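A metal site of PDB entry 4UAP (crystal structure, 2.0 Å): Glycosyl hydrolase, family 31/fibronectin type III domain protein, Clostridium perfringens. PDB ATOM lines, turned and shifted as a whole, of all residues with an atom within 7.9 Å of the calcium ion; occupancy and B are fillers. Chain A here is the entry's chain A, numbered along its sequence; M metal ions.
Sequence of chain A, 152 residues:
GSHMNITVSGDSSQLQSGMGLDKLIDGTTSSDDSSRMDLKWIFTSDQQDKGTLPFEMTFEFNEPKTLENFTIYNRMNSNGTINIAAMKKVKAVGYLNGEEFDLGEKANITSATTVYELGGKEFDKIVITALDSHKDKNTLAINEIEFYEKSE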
ATOM      1  N   GLY A  20     -15.781  22.406  24.656  1.00  0.00           N
ATOM      2  CA  GLY A  20     -15.397  23.799  24.598  1.00  0.00           C
ATOM      3  C   GLY A  20     -15.755  24.518  23.308  1.00  0.00           C
ATOM      4  O   GLY A  20     -16.534  24.013  22.499  1.00  0.00           O
ATOM      5  N   LEU A  21     -15.173  25.694  23.125  1.00  0.00           N
ATOM      6  CA  LEU A  21     -15.485  26.576  21.992  1.00  0.00           C
ATOM      7  C   LEU A  21     -15.302  25.912  20.634  1.00  0.00           C
ATOM      8  O   LEU A  21     -16.016  26.219  19.689  1.00  0.00           O
ATOM      9  CB  LEU A  21     -14.616  27.843  22.073  1.00  0.00           C
ATOM     10  CG  LEU A  21     -14.873  28.743  23.277  1.00  0.00           C
ATOM     11  CD1 LEU A  21     -13.839  29.867  23.377  1.00  0.00           C
ATOM     12  CD2 LEU A  21     -16.265  29.310  23.209  1.00  0.00           C
ATOM     13  N   ASP A  22     -14.332  25.013  20.541  1.00  0.00           N
ATOM     14  CA  ASP A  22     -14.018  24.327  19.301  1.00  0.00           C
ATOM     15  C   ASP A  22     -15.211  23.535  18.765  1.00  0.00           C
ATOM     16  O   ASP A  22     -15.359  23.354  17.562  1.00  0.00           O
ATOM     17  CB  ASP A  22     -12.823  23.396  19.496  1.00  0.00           C
ATOM     18  CG  ASP A  22     -13.065  22.360  20.595  1.00  0.00           C
ATOM     19  OD1 ASP A  22     -13.169  22.746  21.773  1.00  0.00           O
ATOM     20  OD2 ASP A  22     -13.151  21.154  20.272  1.00  0.00           O
ATOM     21  N   LYS A  23     -16.087  23.093  19.678  1.00  0.00           N
ATOM     22  CA  LYS A  23     -17.265  22.309  19.285  1.00  0.00           C
ATOM     23  C   LYS A  23     -18.328  23.168  18.591  1.00  0.00           C
ATOM     24  O   LYS A  23     -19.305  22.649  18.063  1.00  0.00           O
ATOM     25  CB  LYS A  23     -17.869  21.606  20.502  1.00  0.00           C
ATOM     26  CG  LYS A  23     -16.952  20.524  21.113  1.00  0.00           C
ATOM     27  CD  LYS A  23     -16.683  19.406  20.102  1.00  0.00           C
ATOM     28  CE  LYS A  23     -15.746  18.327  20.654  1.00  0.00           C
ATOM     29  NZ  LYS A  23     -16.456  17.355  21.538  1.00  0.00           N
ATOM     30  N   LEU A  24     -18.142  24.485  18.607  1.00  0.00           N
ATOM     31  CA  LEU A  24     -19.058  25.369  17.879  1.00  0.00           C
ATOM     32  C   LEU A  24     -18.755  25.364  16.384  1.00  0.00           C
ATOM     33  O   LEU A  24     -19.615  25.679  15.567  1.00  0.00           O
ATOM     34  CB  LEU A  24     -18.968  26.813  18.400  1.00  0.00           C
ATOM     35  CG  LEU A  24     -19.420  27.092  19.825  1.00  0.00           C
ATOM     36  CD1 LEU A  24     -19.058  28.536  20.242  1.00  0.00           C
ATOM     37  CD2 LEU A  24     -20.929  26.835  19.993  1.00  0.00           C
ATOM     38  N   ILE A  25     -17.529  24.988  16.025  1.00  0.00           N
ATOM     39  CA  ILE A  25     -17.125  25.061  14.622  1.00  0.00           C
ATOM     40  C   ILE A  25     -16.431  23.792  14.126  1.00  0.00           C
ATOM     41  O   ILE A  25     -15.701  23.827  13.127  1.00  0.00           O
ATOM     42  CB  ILE A  25     -16.194  26.277  14.383  1.00  0.00           C
ATOM     43  CG1 ILE A  25     -14.916  26.151  15.212  1.00  0.00           C
ATOM     44  CG2 ILE A  25     -16.891  27.573  14.743  1.00  0.00           C
ATOM     45  CD1 ILE A  25     -13.918  27.263  14.977  1.00  0.00           C
ATOM     46  N   ASP A  26     -16.655  22.666  14.794  1.00  0.00           N
ATOM     47  CA  ASP A  26     -15.964  21.440  14.402  1.00  0.00           C
ATOM     48  C   ASP A  26     -16.689  20.687  13.293  1.00  0.00           C
ATOM     49  O   ASP A  26     -16.243  19.635  12.854  1.00  0.00           O
ATOM     50  CB  ASP A  26     -15.787  20.520  15.609  1.00  0.00           C
ATOM     51  CG  ASP A  26     -17.112  20.055  16.168  1.00  0.00           C
ATOM     52  OD1 ASP A  26     -17.996  20.913  16.362  1.00  0.00           O
ATOM     53  OD2 ASP A  26     -17.278  18.845  16.414  1.00  0.00           O
ATOM     54  N   GLY A  27     -17.817  21.230  12.831  1.00  0.00           N
ATOM     55  CA  GLY A  27     -18.552  20.627  11.730  1.00  0.00           C
ATOM     56  C   GLY A  27     -19.541  19.569  12.179  1.00  0.00           C
ATOM     57  O   GLY A  27     -19.916  18.708  11.397  1.00  0.00           O
ATOM     58  N   THR A  28     -19.954  19.624  13.444  1.00  0.00           N
ATOM     59  CA  THR A  28     -20.929  18.682  13.957  1.00  0.00           C
ATOM     60  C   THR A  28     -22.186  19.398  14.396  1.00  0.00           C
ATOM     61  O   THR A  28     -22.174  20.101  15.411  1.00  0.00           O
ATOM     62  CB  THR A  28     -20.376  17.867  15.160  1.00  0.00           C
ATOM     63  OG1 THR A  28     -19.802  18.762  16.121  1.00  0.00           O
ATOM     64  CG2 THR A  28     -19.310  16.877  14.696  1.00  0.00           C
ATOM     65  N   THR A  29     -23.280  19.207  13.670  1.00  0.00           N
ATOM     66  CA  THR A  29     -24.510  19.935  13.975  1.00  0.00           C
ATOM     67  C   THR A  29     -25.531  19.110  14.749  1.00  0.00           C
ATOM     68  O   THR A  29     -26.599  19.619  15.107  1.00  0.00           O
ATOM     69  CB  THR A  29     -25.181  20.431  12.685  1.00  0.00           C
ATOM     70  OG1 THR A  29     -25.417  19.310  11.818  1.00  0.00           O
ATOM     71  CG2 THR A  29     -24.299  21.445  11.967  1.00  0.00           C
ATOM     72  N   SER A  30     -25.226  17.852  15.020  1.00  0.00           N
ATOM     73  CA  SER A  30     -26.176  17.014  15.763  1.00  0.00           C
ATOM     74  C   SER A  30     -26.215  17.420  17.223  1.00  0.00           C
ATOM     75  O   SER A  30     -25.334  18.148  17.699  1.00  0.00           O
ATOM     76  CB  SER A  30     -25.812  15.532  15.648  1.00  0.00           C
ATOM     77  OG  SER A  30     -24.741  15.222  16.526  1.00  0.00           O
ATOM     78  N   ASP A  32     -25.917  15.400  19.766  1.00  0.00           N
ATOM     79  CA  ASP A  32     -25.149  14.444  20.564  1.00  0.00           C
ATOM     80  C   ASP A  32     -24.190  15.165  21.498  1.00  0.00           C
ATOM     81  O   ASP A  32     -23.696  16.237  21.147  1.00  0.00           O
ATOM     82  CB  ASP A  32     -24.367  13.500  19.641  1.00  0.00           C
ATOM     83  CG  ASP A  32     -25.271  12.657  18.748  1.00  0.00           C
ATOM     84  OD1 ASP A  32     -26.179  11.981  19.272  1.00  0.00           O
ATOM     85  OD2 ASP A  32     -25.088  12.681  17.508  1.00  0.00           O
ATOM     86  N   ASP A  33     -23.902  14.585  22.668  1.00  0.00           N
ATOM     87  CA  ASP A  33     -22.950  15.180  23.609  1.00  0.00           C
ATOM     88  C   ASP A  33     -21.618  15.480  22.918  1.00  0.00           C
ATOM     89  O   ASP A  33     -20.965  16.489  23.233  1.00  0.00           O
ATOM     90  CB  ASP A  33     -22.682  14.261  24.799  1.00  0.00           C
ATOM     91  CG  ASP A  33     -23.852  14.158  25.757  1.00  0.00           C
ATOM     92  OD1 ASP A  33     -24.788  14.980  25.664  1.00  0.00           O
ATOM     93  OD2 ASP A  33     -23.826  13.263  26.632  1.00  0.00           O
ATOM     94  N   SER A  34     -21.220  14.609  22.004  1.00  0.00           N
ATOM     95  CA  SER A  34     -19.919  14.730  21.351  1.00  0.00           C
ATOM     96  C   SER A  34     -19.848  15.880  20.342  1.00  0.00           C
ATOM     97  O   SER A  34     -18.757  16.245  19.889  1.00  0.00           O
ATOM     98  CB  SER A  34     -19.566  13.414  20.668  1.00  0.00           C
ATOM     99  OG  SER A  34     -20.534  13.094  19.679  1.00  0.00           O
ATOM    100  N   SER A  35     -20.999  16.459  19.990  1.00  0.00           N
ATOM    101  CA  SER A  35     -21.049  17.577  19.029  1.00  0.00           C
ATOM    102  C   SER A  35     -21.009  18.967  19.673  1.00  0.00           C
ATOM    103  O   SER A  35     -20.656  19.959  19.023  1.00  0.00           O
ATOM    104  CB  SER A  35     -22.317  17.495  18.164  1.00  0.00           C
ATOM    105  OG  SER A  35     -22.421  16.262  17.471  1.00  0.00           O
ATOM    106  N   ARG A  36     -21.404  19.050  20.941  1.00  0.00           N
ATOM    107  CA  ARG A  36     -21.818  20.321  21.530  1.00  0.00           C
ATOM    108  C   ARG A  36     -20.766  21.086  22.318  1.00  0.00           C
ATOM    109  O   ARG A  36     -19.832  20.495  22.862  1.00  0.00           O
ATOM    110  CB  ARG A  36     -23.018  20.091  22.470  1.00  0.00           C
ATOM    111  CG  ARG A  36     -24.227  19.409  21.852  1.00  0.00           C
ATOM    112  CD  ARG A  36     -25.445  19.596  22.750  1.00  0.00           C
ATOM    113  NE  ARG A  36     -25.117  19.318  24.147  1.00  0.00           N
ATOM    114  CZ  ARG A  36     -25.251  18.139  24.737  1.00  0.00           C
ATOM    115  NH1 ARG A  36     -25.739  17.093  24.070  1.00  0.00           N
ATOM    116  NH2 ARG A  36     -24.897  18.001  26.016  1.00  0.00           N
ATOM    117  N   MET A  37     -20.952  22.413  22.374  1.00  0.00           N
ATOM    118  CA  MET A  37     -20.381  23.262  23.411  1.00  0.00           C
ATOM    119  C   MET A  37     -21.419  23.395  24.528  1.00  0.00           C
ATOM    120  O   MET A  37     -22.555  23.780  24.274  1.00  0.00           O
ATOM    121  CB  MET A  37     -20.021  24.650  22.858  1.00  0.00           C
ATOM    122  CG  MET A  37     -19.346  25.605  23.869  1.00  0.00           C
ATOM    123  SD  MET A  37     -19.706  27.373  23.657  1.00  0.00           S
ATOM    124  CE  MET A  37     -21.334  27.384  24.395  1.00  0.00           C
ATOM    125  N   TYR A  73     -27.142  26.191  15.701  1.00  0.00           N
ATOM    126  CA  TYR A  73     -27.837  24.919  15.828  1.00  0.00           C
ATOM    127  C   TYR A  73     -28.067  24.606  17.302  1.00  0.00           C
ATOM    128  O   TYR A  73     -27.122  24.462  18.087  1.00  0.00           O
ATOM    129  CB  TYR A  73     -27.045  23.812  15.149  1.00  0.00           C
ATOM    130  CG  TYR A  73     -27.005  23.935  13.635  1.00  0.00           C
ATOM    131  CD1 TYR A  73     -26.093  24.782  13.009  1.00  0.00           C
ATOM    132  CD2 TYR A  73     -27.887  23.209  12.835  1.00  0.00           C
ATOM    133  CE1 TYR A  73     -26.056  24.899  11.633  1.00  0.00           C
ATOM    134  CE2 TYR A  73     -27.866  23.327  11.454  1.00  0.00           C
ATOM    135  CZ  TYR A  73     -26.947  24.161  10.857  1.00  0.00           C
ATOM    136  OH  TYR A  73     -26.914  24.271   9.492  1.00  0.00           O
ATOM    137  N   ILE A 142     -25.055  24.330  22.923  1.00  0.00           N
ATOM    138  CA  ILE A 142     -25.122  24.721  21.525  1.00  0.00           C
ATOM    139  C   ILE A 142     -24.398  23.686  20.676  1.00  0.00           C
ATOM    140  O   ILE A 142     -23.266  23.326  20.983  1.00  0.00           O
ATOM    141  CB  ILE A 142     -24.512  26.127  21.304  1.00  0.00           C
ATOM    142  CG1 ILE A 142     -25.274  27.177  22.122  1.00  0.00           C
ATOM    143  CG2 ILE A 142     -24.490  26.480  19.818  1.00  0.00           C
ATOM    144  CD1 ILE A 142     -24.606  28.585  22.113  1.00  0.00           C
ATOM    145  N   ASN A 143     -25.038  23.194  19.615  1.00  0.00           N
ATOM    146  CA  ASN A 143     -24.433  22.180  18.759  1.00  0.00           C
ATOM    147  C   ASN A 143     -23.331  22.730  17.856  1.00  0.00           C
ATOM    148  O   ASN A 143     -22.305  22.098  17.662  1.00  0.00           O
ATOM    149  CB  ASN A 143     -25.494  21.523  17.864  1.00  0.00           C
ATOM    150  CG  ASN A 143     -26.605  20.888  18.637  1.00  0.00           C
ATOM    151  OD1 ASN A 143     -26.557  20.807  19.871  1.00  0.00           O
ATOM    152  ND2 ASN A 143     -27.625  20.410  17.932  1.00  0.00           N
ATOM    153  N   GLU A 144     -23.584  23.889  17.270  1.00  0.00           N
ATOM    154  CA  GLU A 144     -22.731  24.387  16.194  1.00  0.00           C
ATOM    155  C   GLU A 144     -23.195  25.769  15.830  1.00  0.00           C
ATOM    156  O   GLU A 144     -24.374  26.095  15.989  1.00  0.00           O
ATOM    157  CB  GLU A 144     -22.798  23.460  14.954  1.00  0.00           C
ATOM    158  CG  GLU A 144     -21.775  23.804  13.843  1.00  0.00           C
ATOM    159  CD  GLU A 144     -20.439  23.076  14.008  1.00  0.00           C
ATOM    160  OE1 GLU A 144     -19.549  23.215  13.145  1.00  0.00           O
ATOM    161  OE2 GLU A 144     -20.262  22.358  15.019  1.00  0.00           O
ATOM    162  N   ILE A 145     -22.274  26.603  15.359  1.00  0.00           N
ATOM    163  CA  ILE A 145     -22.646  27.866  14.742  1.00  0.00           C
ATOM    164  C   ILE A 145     -21.936  27.918  13.403  1.00  0.00           C
ATOM    165  O   ILE A 145     -20.716  27.750  13.340  1.00  0.00           O
ATOM    166  CB  ILE A 145     -22.265  29.080  15.623  1.00  0.00           C
ATOM    167  CG1 ILE A 145     -23.036  29.018  16.960  1.00  0.00           C
ATOM    168  CG2 ILE A 145     -22.579  30.381  14.871  1.00  0.00           C
ATOM    169  CD1 ILE A 145     -22.673  30.134  17.976  1.00  0.00           C
HETATM  170 CA    CA M   1     -20.414  21.029  16.908  1.00  0.00          CA
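The backbone carbonyl oxygen (O) of Ser 34 is in hydrogen-bond range of the side-chain amino group (NZ) of Lys 23 (3.0 Å).
The side-chain amide nitrogen (ND2) of Asn 143 sits at hydrogen-bond distance from the backbone carbonyl oxygen (O) of Thr 29, 3.1 Å away.
The side-chain amide nitrogen of Asn 143 sits close to the backbone carbonyl oxygen of Ser 30, 3.2 Å away.
The backbone NH (N) of Asn 143 sits at hydrogen-bond distance from the backbone carbonyl oxygen (O) of Tyr 73 (2.9 Å).
N of Gly 27 sits at hydrogen-bond distance from OE1 of Glu 144 (2.7 Å).
The backbone carbonyl oxygen (O) of Glu 144 sits at hydrogen-bond distance from the backbone NH (N) of Tyr 73, at 2.8 Å.
The side-chain hydroxyl (OG) of Ser 35 sits at hydrogen-bond distance from the side-chain hydroxyl (OG) of Ser 30 (2.7 Å).
Along chain A the residues within 4 Å of the calcium ion span positions 23 to 144.
O of Lys 23 is bound to the calcium ion (2.3 Å).
O of Asn 143 is bound to the calcium ion, at 2.3 Å.
The calcium ion is bound by OE2 of Glu 144 (2.3 Å).
The calcium ion is bound by the backbone carbonyl oxygen (O) of Ser 35, 2.4 Å away.
The calcium ion is bound by OG1 of Thr 28.
The calcium ion is bound by OD1 of Asp 26 (2.5 Å).
The backbone carbonyl oxygen (O) of Thr 28 is bound to the calcium ion (2.5 Å).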
